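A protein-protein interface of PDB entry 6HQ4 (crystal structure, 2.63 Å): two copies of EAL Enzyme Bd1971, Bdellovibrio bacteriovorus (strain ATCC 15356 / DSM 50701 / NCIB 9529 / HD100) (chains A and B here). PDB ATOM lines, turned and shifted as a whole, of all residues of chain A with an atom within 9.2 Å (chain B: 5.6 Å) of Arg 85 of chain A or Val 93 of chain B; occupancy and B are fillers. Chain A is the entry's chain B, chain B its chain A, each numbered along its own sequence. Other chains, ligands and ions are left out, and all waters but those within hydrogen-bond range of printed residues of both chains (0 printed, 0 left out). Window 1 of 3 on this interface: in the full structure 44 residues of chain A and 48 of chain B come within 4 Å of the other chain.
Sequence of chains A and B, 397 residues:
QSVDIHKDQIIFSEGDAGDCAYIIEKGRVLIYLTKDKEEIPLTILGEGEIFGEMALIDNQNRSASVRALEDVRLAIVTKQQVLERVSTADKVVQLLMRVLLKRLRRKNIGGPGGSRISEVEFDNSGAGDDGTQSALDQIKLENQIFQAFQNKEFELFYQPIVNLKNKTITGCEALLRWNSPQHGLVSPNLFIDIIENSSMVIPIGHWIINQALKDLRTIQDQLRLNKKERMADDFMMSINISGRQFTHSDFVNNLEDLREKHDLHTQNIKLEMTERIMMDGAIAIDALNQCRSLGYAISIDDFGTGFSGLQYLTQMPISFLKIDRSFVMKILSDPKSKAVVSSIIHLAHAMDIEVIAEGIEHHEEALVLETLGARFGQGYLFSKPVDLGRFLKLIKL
The side-chain carboxylate (OE1) of Glu 142 of chain B lies within hydrogen-bond range of the side-chain amide nitrogen (NE2) of Gln 81 of chain A (2.9 Å). OD2 of Asp 90 of chain B is in salt-bridge range of NE of Arg 85 of chain A. The side-chain carboxylate (OE1) of Glu 142 of chain B lies within salt-bridge range of the guanidinium group (NH2) of Arg 85 of chain A. The side-chain amide nitrogen (NE2) of Gln 81 of chain A is in hydrogen-bond range of the backbone carbonyl oxygen (O) of Ile 139 of chain B. The side-chain amide oxygen (OE1) of Gln 138 of chain B lies within hydrogen-bond range of the guanidinium group (NH2) of Arg 85 of chain A (2.9 Å).
NH1 of Arg 85 of chain A sits at hydrogen-bond distance from O of Gln 81 of chain A (3.0 Å). The backbone NH (N) of Thr 78 of chain A sits at hydrogen-bond distance from the side-chain amide oxygen (OE1) of Gln 81 of chain A (3.0 Å). The side-chain carboxylate (OD2) of Asp 90 of chain B sits close to the backbone NH (N) of Val 92 of chain B (3.4 Å).
Glu 53 of chain A touches Leu 96 of chain B (CG to CD2, 3.5 Å). Arg 85 of chain A touches Val 92 of chain B. Arg 85 of chain A touches Val 93 of chain B. Arg 85 of chain A touches Ile 139 of chain B. Val 93 of chain B touches Val 93 of chain A (CG1 to CG1, 3.9 Å). CE of Met 97 of chain B touches CD1 of Leu 96 of chain A, 3.6 Å away. CD1 of Leu 96 of chain B touches CE of Met 97 of chain A (3.8 Å).
Asp 90 of chain B touches just one residue of chain A: Arg 85 (3.2 Å). Val 93 of chain B touches two residues of chain A. Printed residues of chain A within 4 Å of Gln 138 of chain B: Arg 85 (2.9 Å). Of the printed residues of chain A, Ile 139 of chain B touches Ile 76, Gln 81 and Arg 85. Printed residues of chain A within 4 Å of Glu 142 of chain B: Gln 81 (2.9 Å) and Arg 85 (3.4 Å). The nearest residue of chain A that does not touch Val 93 of chain B is Val 86 of chain A (4.1 Å). The nearest printed residue of chain A that does not touch Met 97 of chain B is Leu 100 of chain A (4.1 Å).
Of the 25 printed residues of chain A, 7 touch a printed residue of chain B. Among the printed residues, 14 pairs touch across the chains.
Val 93 of chain B touches its own counterpart, Val 93 of chain A. Leu 96 of chain A touches Met 97 of chain B, and with the chains exchanged Met 97 of chain A touches Leu 96 of chain B. Met 97 of chain B touches its own counterpart, Met 97 of chain A. Of the 14 pairs that touch across the chains among the printed residues, 4 have their exchanged pair printed and touching as well.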
ATOM      1  N   ILE A  50      32.860  32.585  -3.787  1.00  0.00           N
ATOM      2  CA  ILE A  50      31.884  32.047  -4.739  1.00  0.00           C
ATOM      3  C   ILE A  50      31.004  33.154  -5.324  1.00  0.00           C
ATOM      4  O   ILE A  50      30.830  34.204  -4.710  1.00  0.00           O
ATOM      5  CB  ILE A  50      30.984  30.991  -4.056  1.00  0.00           C
ATOM      6  CG1 ILE A  50      30.256  30.131  -5.092  1.00  0.00           C
ATOM      7  CG2 ILE A  50      29.984  31.644  -3.109  1.00  0.00           C
ATOM      8  CD1 ILE A  50      29.410  29.033  -4.492  1.00  0.00           C
ATOM      9  N   GLU A  53      25.630  31.874  -7.306  1.00  0.00           N
ATOM     10  CA  GLU A  53      24.952  30.828  -6.548  1.00  0.00           C
ATOM     11  C   GLU A  53      23.491  31.159  -6.223  1.00  0.00           C
ATOM     12  O   GLU A  53      22.691  30.249  -6.011  1.00  0.00           O
ATOM     13  CB  GLU A  53      25.727  30.514  -5.260  1.00  0.00           C
ATOM     14  CG  GLU A  53      25.416  31.390  -4.045  1.00  0.00           C
ATOM     15  CD  GLU A  53      25.792  32.847  -4.215  1.00  0.00           C
ATOM     16  OE1 GLU A  53      26.500  33.177  -5.180  1.00  0.00           O
ATOM     17  OE2 GLU A  53      25.392  33.669  -3.369  1.00  0.00           O
ATOM     18  N   ILE A  57      19.719  28.701  -6.435  1.00  0.00           N
ATOM     19  CA  ILE A  57      18.993  28.268  -5.234  1.00  0.00           C
ATOM     20  C   ILE A  57      17.482  28.518  -5.326  1.00  0.00           C
ATOM     21  O   ILE A  57      16.699  27.665  -4.912  1.00  0.00           O
ATOM     22  CB  ILE A  57      19.563  28.927  -3.957  1.00  0.00           C
ATOM     23  CG1 ILE A  57      21.007  28.467  -3.741  1.00  0.00           C
ATOM     24  CG2 ILE A  57      18.725  28.571  -2.731  1.00  0.00           C
ATOM     25  CD1 ILE A  57      21.803  29.344  -2.803  1.00  0.00           C
ATOM     26  N   ILE A  76      33.830  25.254 -11.734  1.00  0.00           N
ATOM     27  CA  ILE A  76      32.380  25.281 -11.961  1.00  0.00           C
ATOM     28  C   ILE A  76      31.586  24.467 -10.933  1.00  0.00           C
ATOM     29  O   ILE A  76      31.931  23.327 -10.619  1.00  0.00           O
ATOM     30  CB  ILE A  76      32.023  24.808 -13.391  1.00  0.00           C
ATOM     31  CG1 ILE A  76      32.686  25.732 -14.416  1.00  0.00           C
ATOM     32  CG2 ILE A  76      30.507  24.774 -13.598  1.00  0.00           C
ATOM     33  CD1 ILE A  76      32.236  25.524 -15.848  1.00  0.00           C
ATOM     34  N   VAL A  77      30.523  25.085 -10.421  1.00  0.00           N
ATOM     35  CA  VAL A  77      29.524  24.425  -9.590  1.00  0.00           C
ATOM     36  C   VAL A  77      28.213  24.428 -10.376  1.00  0.00           C
ATOM     37  O   VAL A  77      27.686  25.492 -10.695  1.00  0.00           O
ATOM     38  CB  VAL A  77      29.305  25.190  -8.268  1.00  0.00           C
ATOM     39  CG1 VAL A  77      28.250  24.506  -7.425  1.00  0.00           C
ATOM     40  CG2 VAL A  77      30.607  25.321  -7.489  1.00  0.00           C
ATOM     41  N   THR A  78      27.680  23.251 -10.680  1.00  0.00           N
ATOM     42  CA  THR A  78      26.463  23.158 -11.488  1.00  0.00           C
ATOM     43  C   THR A  78      25.223  23.404 -10.636  1.00  0.00           C
ATOM     44  O   THR A  78      25.278  23.350  -9.412  1.00  0.00           O
ATOM     45  CB  THR A  78      26.324  21.788 -12.189  1.00  0.00           C
ATOM     46  OG1 THR A  78      26.075  20.761 -11.223  1.00  0.00           O
ATOM     47  CG2 THR A  78      27.584  21.456 -12.984  1.00  0.00           C
ATOM     48  N   LYS A  79      24.108  23.665 -11.308  1.00  0.00           N
ATOM     49  CA  LYS A  79      22.819  23.864 -10.651  1.00  0.00           C
ATOM     50  C   LYS A  79      22.410  22.622  -9.877  1.00  0.00           C
ATOM     51  O   LYS A  79      21.970  22.703  -8.727  1.00  0.00           O
ATOM     52  CB  LYS A  79      21.753  24.199 -11.696  1.00  0.00           C
ATOM     53  CG  LYS A  79      20.420  24.655 -11.122  1.00  0.00           C
ATOM     54  CD  LYS A  79      19.565  25.335 -12.185  1.00  0.00           C
ATOM     55  CE  LYS A  79      18.469  26.184 -11.558  1.00  0.00           C
ATOM     56  NZ  LYS A  79      17.644  26.887 -12.579  1.00  0.00           N
ATOM     57  N   GLN A  80      22.574  21.470 -10.516  1.00  0.00           N
ATOM     58  CA  GLN A  80      22.188  20.200  -9.917  1.00  0.00           C
ATOM     59  C   GLN A  80      22.978  19.905  -8.646  1.00  0.00           C
ATOM     60  O   GLN A  80      22.422  19.402  -7.668  1.00  0.00           O
ATOM     61  CB  GLN A  80      22.368  19.068 -10.931  1.00  0.00           C
ATOM     62  CG  GLN A  80      21.798  17.736 -10.487  1.00  0.00           C
ATOM     63  CD  GLN A  80      20.340  17.827 -10.060  1.00  0.00           C
ATOM     64  OE1 GLN A  80      19.578  18.649 -10.581  1.00  0.00           O
ATOM     65  NE2 GLN A  80      19.943  16.976  -9.112  1.00  0.00           N
ATOM     66  N   GLN A  81      24.269  20.222  -8.661  1.00  0.00           N
ATOM     67  CA  GLN A  81      25.109  20.065  -7.473  1.00  0.00           C
ATOM     68  C   GLN A  81      24.615  20.918  -6.296  1.00  0.00           C
ATOM     69  O   GLN A  81      24.620  20.454  -5.152  1.00  0.00           O
ATOM     70  CB  GLN A  81      26.565  20.408  -7.797  1.00  0.00           C
ATOM     71  CG  GLN A  81      27.270  19.335  -8.618  1.00  0.00           C
ATOM     72  CD  GLN A  81      28.686  19.702  -9.029  1.00  0.00           C
ATOM     73  OE1 GLN A  81      28.925  20.773  -9.599  1.00  0.00           O
ATOM     74  NE2 GLN A  81      29.633  18.804  -8.758  1.00  0.00           N
ATOM     75  N   VAL A  82      24.181  22.148  -6.585  1.00  0.00           N
ATOM     76  CA  VAL A  82      23.688  23.069  -5.550  1.00  0.00           C
ATOM     77  C   VAL A  82      22.335  22.637  -4.983  1.00  0.00           C
ATOM     78  O   VAL A  82      22.181  22.533  -3.767  1.00  0.00           O
ATOM     79  CB  VAL A  82      23.580  24.520  -6.079  1.00  0.00           C
ATOM     80  CG1 VAL A  82      22.889  25.430  -5.066  1.00  0.00           C
ATOM     81  CG2 VAL A  82      24.959  25.059  -6.401  1.00  0.00           C
ATOM     82  N   LEU A  83      21.362  22.409  -5.865  1.00  0.00           N
ATOM     83  CA  LEU A  83      20.014  21.985  -5.461  1.00  0.00           C
ATOM     84  C   LEU A  83      20.057  20.659  -4.688  1.00  0.00           C
ATOM     85  O   LEU A  83      19.372  20.488  -3.665  1.00  0.00           O
ATOM     86  CB  LEU A  83      19.102  21.845  -6.696  1.00  0.00           C
ATOM     87  CG  LEU A  83      18.601  23.058  -7.534  1.00  0.00           C
ATOM     88  CD1 LEU A  83      17.478  22.551  -8.431  1.00  0.00           C
ATOM     89  CD2 LEU A  83      18.117  24.264  -6.738  1.00  0.00           C
ATOM     90  N   GLU A  84      20.873  19.733  -5.186  1.00  0.00           N
ATOM     91  CA  GLU A  84      21.111  18.448  -4.531  1.00  0.00           C
ATOM     92  C   GLU A  84      21.491  18.615  -3.058  1.00  0.00           C
ATOM     93  O   GLU A  84      20.933  17.947  -2.189  1.00  0.00           O
ATOM     94  CB  GLU A  84      22.220  17.701  -5.277  1.00  0.00           C
ATOM     95  CG  GLU A  84      22.620  16.360  -4.677  1.00  0.00           C
ATOM     96  CD  GLU A  84      21.534  15.309  -4.807  1.00  0.00           C
ATOM     97  OE1 GLU A  84      21.190  14.951  -5.954  1.00  0.00           O
ATOM     98  OE2 GLU A  84      21.038  14.828  -3.765  1.00  0.00           O
ATOM     99  N   ARG A  85      22.446  19.498  -2.786  1.00  0.00           N
ATOM    100  CA  ARG A  85      22.945  19.709  -1.423  1.00  0.00           C
ATOM    101  C   ARG A  85      21.994  20.530  -0.555  1.00  0.00           C
ATOM    102  O   ARG A  85      21.865  20.263   0.640  1.00  0.00           O
ATOM    103  CB  ARG A  85      24.325  20.365  -1.453  1.00  0.00           C
ATOM    104  CG  ARG A  85      25.406  19.412  -1.923  1.00  0.00           C
ATOM    105  CD  ARG A  85      26.637  20.139  -2.427  1.00  0.00           C
ATOM    106  NE  ARG A  85      27.716  19.191  -2.710  1.00  0.00           N
ATOM    107  CZ  ARG A  85      27.789  18.414  -3.791  1.00  0.00           C
ATOM    108  NH1 ARG A  85      26.856  18.459  -4.737  1.00  0.00           N
ATOM    109  NH2 ARG A  85      28.817  17.585  -3.933  1.00  0.00           N
ATOM    110  N   VAL A  86      21.333  21.515  -1.159  1.00  0.00           N
ATOM    111  CA  VAL A  86      20.352  22.344  -0.454  1.00  0.00           C
ATOM    112  C   VAL A  86      19.122  21.533  -0.040  1.00  0.00           C
ATOM    113  O   VAL A  86      18.584  21.736   1.047  1.00  0.00           O
ATOM    114  CB  VAL A  86      19.925  23.563  -1.310  1.00  0.00           C
ATOM    115  CG1 VAL A  86      18.687  24.248  -0.741  1.00  0.00           C
ATOM    116  CG2 VAL A  86      21.071  24.560  -1.406  1.00  0.00           C
ATOM    117  N   SER A  87      18.689  20.619  -0.904  1.00  0.00           N
ATOM    118  CA  SER A  87      17.492  19.815  -0.646  1.00  0.00           C
ATOM    119  C   SER A  87      17.643  18.852   0.536  1.00  0.00           C
ATOM    120  O   SER A  87      16.703  18.672   1.309  1.00  0.00           O
ATOM    121  CB  SER A  87      17.092  19.043  -1.907  1.00  0.00           C
ATOM    122  OG  SER A  87      18.194  18.338  -2.450  1.00  0.00           O
ATOM    123  N   THR A  88      18.816  18.238   0.676  1.00  0.00           N
ATOM    124  CA  THR A  88      19.076  17.337   1.809  1.00  0.00           C
ATOM    125  C   THR A  88      19.316  18.043   3.139  1.00  0.00           C
ATOM    126  O   THR A  88      19.250  17.401   4.187  1.00  0.00           O
ATOM    127  CB  THR A  88      20.297  16.424   1.579  1.00  0.00           C
ATOM    128  OG1 THR A  88      21.495  17.211   1.542  1.00  0.00           O
ATOM    129  CG2 THR A  88      20.149  15.623   0.291  1.00  0.00           C
ATOM    130  N   ALA A  89      19.617  19.342   3.104  1.00  0.00           N
ATOM    131  CA  ALA A  89      19.888  20.102   4.328  1.00  0.00           C
ATOM    132  C   ALA A  89      18.647  20.201   5.211  1.00  0.00           C
ATOM    133  O   ALA A  89      17.518  20.148   4.721  1.00  0.00           O
ATOM    134  CB  ALA A  89      20.406  21.491   3.991  1.00  0.00           C
ATOM    135  N   ASP A  90      18.873  20.345   6.514  1.00  0.00           N
ATOM    136  CA  ASP A  90      17.792  20.450   7.500  1.00  0.00           C
ATOM    137  C   ASP A  90      16.773  21.533   7.115  1.00  0.00           C
ATOM    138  O   ASP A  90      17.129  22.559   6.532  1.00  0.00           O
ATOM    139  CB  ASP A  90      18.379  20.750   8.882  1.00  0.00           C
ATOM    140  CG  ASP A  90      17.326  20.794   9.967  1.00  0.00           C
ATOM    141  OD1 ASP A  90      16.550  19.823  10.083  1.00  0.00           O
ATOM    142  OD2 ASP A  90      17.272  21.799  10.704  1.00  0.00           O
ATOM    143  N   VAL A  92      15.194  23.742   8.798  1.00  0.00           N
ATOM    144  CA  VAL A  92      15.478  25.048   9.403  1.00  0.00           C
ATOM    145  C   VAL A  92      16.628  25.737   8.678  1.00  0.00           C
ATOM    146  O   VAL A  92      16.585  26.943   8.442  1.00  0.00           O
ATOM    147  CB  VAL A  92      15.832  24.917  10.901  1.00  0.00           C
ATOM    148  CG1 VAL A  92      16.245  26.261  11.487  1.00  0.00           C
ATOM    149  CG2 VAL A  92      14.657  24.336  11.675  1.00  0.00           C
ATOM    150  N   VAL A  93      17.653  24.968   8.327  1.00  0.00           N
ATOM    151  CA  VAL A  93      18.777  25.488   7.539  1.00  0.00           C
ATOM    152  C   VAL A  93      18.308  25.974   6.156  1.00  0.00           C
ATOM    153  O   VAL A  93      18.869  26.920   5.604  1.00  0.00           O
ATOM    154  CB  VAL A  93      19.901  24.432   7.416  1.00  0.00           C
ATOM    155  CG1 VAL A  93      20.954  24.853   6.402  1.00  0.00           C
ATOM    156  CG2 VAL A  93      20.544  24.197   8.775  1.00  0.00           C
ATOM    157  N   GLN A  94      17.272  25.341   5.609  1.00  0.00           N
ATOM    158  CA  GLN A  94      16.670  25.801   4.357  1.00  0.00           C
ATOM    159  C   GLN A  94      15.873  27.096   4.556  1.00  0.00           C
ATOM    160  O   GLN A  94      15.957  27.999   3.727  1.00  0.00           O
ATOM    161  CB  GLN A  94      15.797  24.706   3.732  1.00  0.00           C
ATOM    162  CG  GLN A  94      16.605  23.507   3.251  1.00  0.00           C
ATOM    163  CD  GLN A  94      15.800  22.522   2.422  1.00  0.00           C
ATOM    164  OE1 GLN A  94      14.976  22.913   1.595  1.00  0.00           O
ATOM    165  NE2 GLN A  94      16.046  21.230   2.628  1.00  0.00           N
ATOM    166  N   LEU A  95      15.104  27.178   5.646  1.00  0.00           N
ATOM    167  CA  LEU A  95      14.423  28.421   6.031  1.00  0.00           C
ATOM    168  C   LEU A  95      15.440  29.553   6.092  1.00  0.00           C
ATOM    169  O   LEU A  95      15.238  30.606   5.493  1.00  0.00           O
ATOM    170  CB  LEU A  95      13.717  28.274   7.393  1.00  0.00           C
ATOM    171  CG  LEU A  95      13.090  29.525   8.088  1.00  0.00           C
ATOM    172  CD1 LEU A  95      11.869  29.167   8.940  1.00  0.00           C
ATOM    173  CD2 LEU A  95      14.092  30.294   8.950  1.00  0.00           C
ATOM    174  N   LEU A  96      16.529  29.319   6.823  1.00  0.00           N
ATOM    175  CA  LEU A  96      17.596  30.310   6.997  1.00  0.00           C
ATOM    176  C   LEU A  96      18.161  30.803   5.663  1.00  0.00           C
ATOM    177  O   LEU A  96      18.334  32.005   5.460  1.00  0.00           O
ATOM    178  CB  LEU A  96      18.731  29.735   7.858  1.00  0.00           C
ATOM    179  CG  LEU A  96      18.421  29.480   9.336  1.00  0.00           C
ATOM    180  CD1 LEU A  96      19.598  28.805  10.024  1.00  0.00           C
ATOM    181  CD2 LEU A  96      18.060  30.772  10.048  1.00  0.00           C
ATOM    182  N   MET A  97      18.445  29.868   4.762  1.00  0.00           N
ATOM    183  CA  MET A  97      18.952  30.206   3.434  1.00  0.00           C
ATOM    184  C   MET A  97      17.980  31.097   2.673  1.00  0.00           C
ATOM    185  O   MET A  97      18.366  32.142   2.153  1.00  0.00           O
ATOM    186  CB  MET A  97      19.204  28.933   2.626  1.00  0.00           C
ATOM    187  CG  MET A  97      20.494  28.227   2.997  1.00  0.00           C
ATOM    188  SD  MET A  97      21.881  28.837   2.021  1.00  0.00           S
ATOM    189  CE  MET A  97      21.611  27.918   0.504  1.00  0.00           C
ATOM    190  N   LEU A 100      17.628  34.723   3.954  1.00  0.00           N
ATOM    191  CA  LEU A 100      18.815  35.527   3.646  1.00  0.00           C
ATOM    192  C   LEU A 100      18.852  35.973   2.182  1.00  0.00           C
ATOM    193  O   LEU A 100      19.300  37.080   1.889  1.00  0.00           O
ATOM    194  CB  LEU A 100      20.098  34.767   3.989  1.00  0.00           C
ATOM    195  CG  LEU A 100      20.401  34.581   5.478  1.00  0.00           C
ATOM    196  CD1 LEU A 100      21.532  33.580   5.660  1.00  0.00           C
ATOM    197  CD2 LEU A 100      20.739  35.904   6.151  1.00  0.00           C
ATOM    198  N   ALA B  89      24.965  20.514   8.631  1.00  0.00           N
ATOM    199  CA  ALA B  89      24.701  20.761   7.211  1.00  0.00           C
ATOM    200  C   ALA B  89      25.956  20.580   6.354  1.00  0.00           C
ATOM    201  O   ALA B  89      27.076  20.746   6.835  1.00  0.00           O
ATOM    202  CB  ALA B  89      24.126  22.156   7.017  1.00  0.00           C
ATOM    203  N   ASP B  90      25.754  20.240   5.083  1.00  0.00           N
ATOM    204  CA  ASP B  90      26.853  20.029   4.131  1.00  0.00           C
ATOM    205  C   ASP B  90      27.828  21.212   4.099  1.00  0.00           C
ATOM    206  O   ASP B  90      27.422  22.363   4.271  1.00  0.00           O
ATOM    207  CB  ASP B  90      26.285  19.790   2.729  1.00  0.00           C
ATOM    208  CG  ASP B  90      27.357  19.483   1.706  1.00  0.00           C
ATOM    209  OD1 ASP B  90      28.169  18.564   1.945  1.00  0.00           O
ATOM    210  OD2 ASP B  90      27.388  20.158   0.658  1.00  0.00           O
ATOM    211  N   LYS B  91      29.107  20.916   3.871  1.00  0.00           N
ATOM    212  CA  LYS B  91      30.172  21.928   3.901  1.00  0.00           C
ATOM    213  C   LYS B  91      29.957  23.059   2.881  1.00  0.00           C
ATOM    214  O   LYS B  91      30.319  24.208   3.141  1.00  0.00           O
ATOM    215  CB  LYS B  91      31.544  21.265   3.685  1.00  0.00           C
ATOM    216  CG  LYS B  91      32.740  22.155   4.019  1.00  0.00           C
ATOM    217  CD  LYS B  91      34.085  21.592   3.577  1.00  0.00           C
ATOM    218  CE  LYS B  91      34.519  20.386   4.400  1.00  0.00           C
ATOM    219  NZ  LYS B  91      35.994  20.185   4.327  1.00  0.00           N
ATOM    220  N   VAL B  92      29.365  22.730   1.733  1.00  0.00           N
ATOM    221  CA  VAL B  92      29.043  23.723   0.700  1.00  0.00           C
ATOM    222  C   VAL B  92      27.859  24.584   1.135  1.00  0.00           C
ATOM    223  O   VAL B  92      27.852  25.795   0.918  1.00  0.00           O
ATOM    224  CB  VAL B  92      28.712  23.056  -0.653  1.00  0.00           C
ATOM    225  CG1 VAL B  92      28.260  24.088  -1.681  1.00  0.00           C
ATOM    226  CG2 VAL B  92      29.910  22.276  -1.175  1.00  0.00           C
ATOM    227  N   VAL B  93      26.855  23.950   1.738  1.00  0.00           N
ATOM    228  CA  VAL B  93      25.698  24.667   2.280  1.00  0.00           C
ATOM    229  C   VAL B  93      26.123  25.632   3.398  1.00  0.00           C
ATOM    230  O   VAL B  93      25.515  26.688   3.575  1.00  0.00           O
ATOM    231  CB  VAL B  93      24.607  23.683   2.765  1.00  0.00           C
ATOM    232  CG1 VAL B  93      23.518  24.395   3.555  1.00  0.00           C
ATOM    233  CG2 VAL B  93      23.998  22.953   1.574  1.00  0.00           C
ATOM    234  N   GLN B  94      27.172  25.279   4.137  1.00  0.00           N
ATOM    235  CA  GLN B  94      27.731  26.179   5.147  1.00  0.00           C
ATOM    236  C   GLN B  94      28.480  27.346   4.511  1.00  0.00           C
ATOM    237  O   GLN B  94      28.342  28.486   4.956  1.00  0.00           O
ATOM    238  CB  GLN B  94      28.633  25.416   6.120  1.00  0.00           C
ATOM    239  CG  GLN B  94      27.858  24.437   6.991  1.00  0.00           C
ATOM    240  CD  GLN B  94      28.682  23.849   8.124  1.00  0.00           C
ATOM    241  OE1 GLN B  94      29.477  24.543   8.757  1.00  0.00           O
ATOM    242  NE2 GLN B  94      28.476  22.563   8.401  1.00  0.00           N
ATOM    243  N   LEU B  95      29.264  27.064   3.472  1.00  0.00           N
ATOM    244  CA  LEU B  95      29.902  28.111   2.673  1.00  0.00           C
ATOM    245  C   LEU B  95      28.852  29.108   2.188  1.00  0.00           C
ATOM    246  O   LEU B  95      29.001  30.316   2.372  1.00  0.00           O
ATOM    247  CB  LEU B  95      30.641  27.503   1.473  1.00  0.00           C
ATOM    248  CG  LEU B  95      31.264  28.435   0.437  1.00  0.00           C
ATOM    249  CD1 LEU B  95      32.202  29.432   1.095  1.00  0.00           C
ATOM    250  CD2 LEU B  95      31.993  27.646  -0.640  1.00  0.00           C
ATOM    251  N   LEU B  96      27.786  28.586   1.583  1.00  0.00           N
ATOM    252  CA  LEU B  96      26.686  29.411   1.072  1.00  0.00           C
ATOM    253  C   LEU B  96      26.080  30.320   2.149  1.00  0.00           C
ATOM    254  O   LEU B  96      25.847  31.505   1.913  1.00  0.00           O
ATOM    255  CB  LEU B  96      25.590  28.524   0.472  1.00  0.00           C
ATOM    256  CG  LEU B  96      25.932  27.775  -0.818  1.00  0.00           C
ATOM    257  CD1 LEU B  96      24.793  26.852  -1.224  1.00  0.00           C
ATOM    258  CD2 LEU B  96      26.254  28.748  -1.941  1.00  0.00           C
ATOM    259  N   MET B  97      25.825  29.757   3.327  1.00  0.00           N
ATOM    260  CA  MET B  97      25.279  30.522   4.446  1.00  0.00           C
ATOM    261  C   MET B  97      26.199  31.670   4.857  1.00  0.00           C
ATOM    262  O   MET B  97      25.758  32.818   4.962  1.00  0.00           O
ATOM    263  CB  MET B  97      25.035  29.605   5.646  1.00  0.00           C
ATOM    264  CG  MET B  97      23.778  28.763   5.525  1.00  0.00           C
ATOM    265  SD  MET B  97      22.326  29.610   6.164  1.00  0.00           S
ATOM    266  CE  MET B  97      22.528  29.333   7.918  1.00  0.00           C
ATOM    267  N   ARG B  98      27.473  31.352   5.079  1.00  0.00           N
ATOM    268  CA  ARG B  98      28.443  32.336   5.562  1.00  0.00           C
ATOM    269  C   ARG B  98      28.623  33.504   4.576  1.00  0.00           C
ATOM    270  O   ARG B  98      28.665  34.667   4.986  1.00  0.00           O
ATOM    271  CB  ARG B  98      29.792  31.675   5.931  1.00  0.00           C
ATOM    272  CG  ARG B  98      29.764  30.845   7.212  1.00  0.00           C
ATOM    273  CD  ARG B  98      31.106  30.187   7.514  1.00  0.00           C
ATOM    274  NE  ARG B  98      31.419  29.082   6.606  1.00  0.00           N
ATOM    275  CZ  ARG B  98      32.533  28.351   6.650  1.00  0.00           C
ATOM    276  NH1 ARG B  98      33.473  28.591   7.559  1.00  0.00           N
ATOM    277  NH2 ARG B  98      32.711  27.369   5.772  1.00  0.00           N
ATOM    278  N   GLN B 138      35.539  17.419  -3.858  1.00  0.00           N
ATOM    279  CA  GLN B 138      34.394  16.522  -4.113  1.00  0.00           C
ATOM    280  C   GLN B 138      33.598  16.986  -5.335  1.00  0.00           C
ATOM    281  O   GLN B 138      33.169  16.168  -6.146  1.00  0.00           O
ATOM    282  CB  GLN B 138      33.458  16.392  -2.883  1.00  0.00           C
ATOM    283  CG  GLN B 138      32.297  17.394  -2.818  1.00  0.00           C
ATOM    284  CD  GLN B 138      31.443  17.363  -1.546  1.00  0.00           C
ATOM    285  OE1 GLN B 138      30.384  17.988  -1.529  1.00  0.00           O
ATOM    286  NE2 GLN B 138      31.879  16.658  -0.493  1.00  0.00           N
ATOM    287  N   ILE B 139      33.411  18.301  -5.449  1.00  0.00           N
ATOM    288  CA  ILE B 139      32.678  18.912  -6.558  1.00  0.00           C
ATOM    289  C   ILE B 139      33.425  18.723  -7.888  1.00  0.00           C
ATOM    290  O   ILE B 139      32.809  18.418  -8.907  1.00  0.00           O
ATOM    291  CB  ILE B 139      32.410  20.420  -6.283  1.00  0.00           C
ATOM    292  CG1 ILE B 139      31.351  20.573  -5.150  1.00  0.00           C
ATOM    293  CG2 ILE B 139      32.061  21.162  -7.580  1.00  0.00           C
ATOM    294  CD1 ILE B 139      29.899  20.423  -5.568  1.00  0.00           C
ATOM    295  N   GLU B 142      33.432  14.942  -9.119  1.00  0.00           N
ATOM    296  CA  GLU B 142      32.109  14.666  -9.695  1.00  0.00           C
ATOM    297  C   GLU B 142      32.017  15.087 -11.161  1.00  0.00           C
ATOM    298  O   GLU B 142      31.478  14.362 -11.985  1.00  0.00           O
ATOM    299  CB  GLU B 142      31.008  15.376  -8.889  1.00  0.00           C
ATOM    300  CG  GLU B 142      30.603  14.639  -7.623  1.00  0.00           C
ATOM    301  CD  GLU B 142      29.470  15.307  -6.870  1.00  0.00           C
ATOM    302  OE1 GLU B 142      29.156  16.479  -7.162  1.00  0.00           O
ATOM    303  OE2 GLU B 142      28.892  14.658  -5.972  1.00  0.00           O
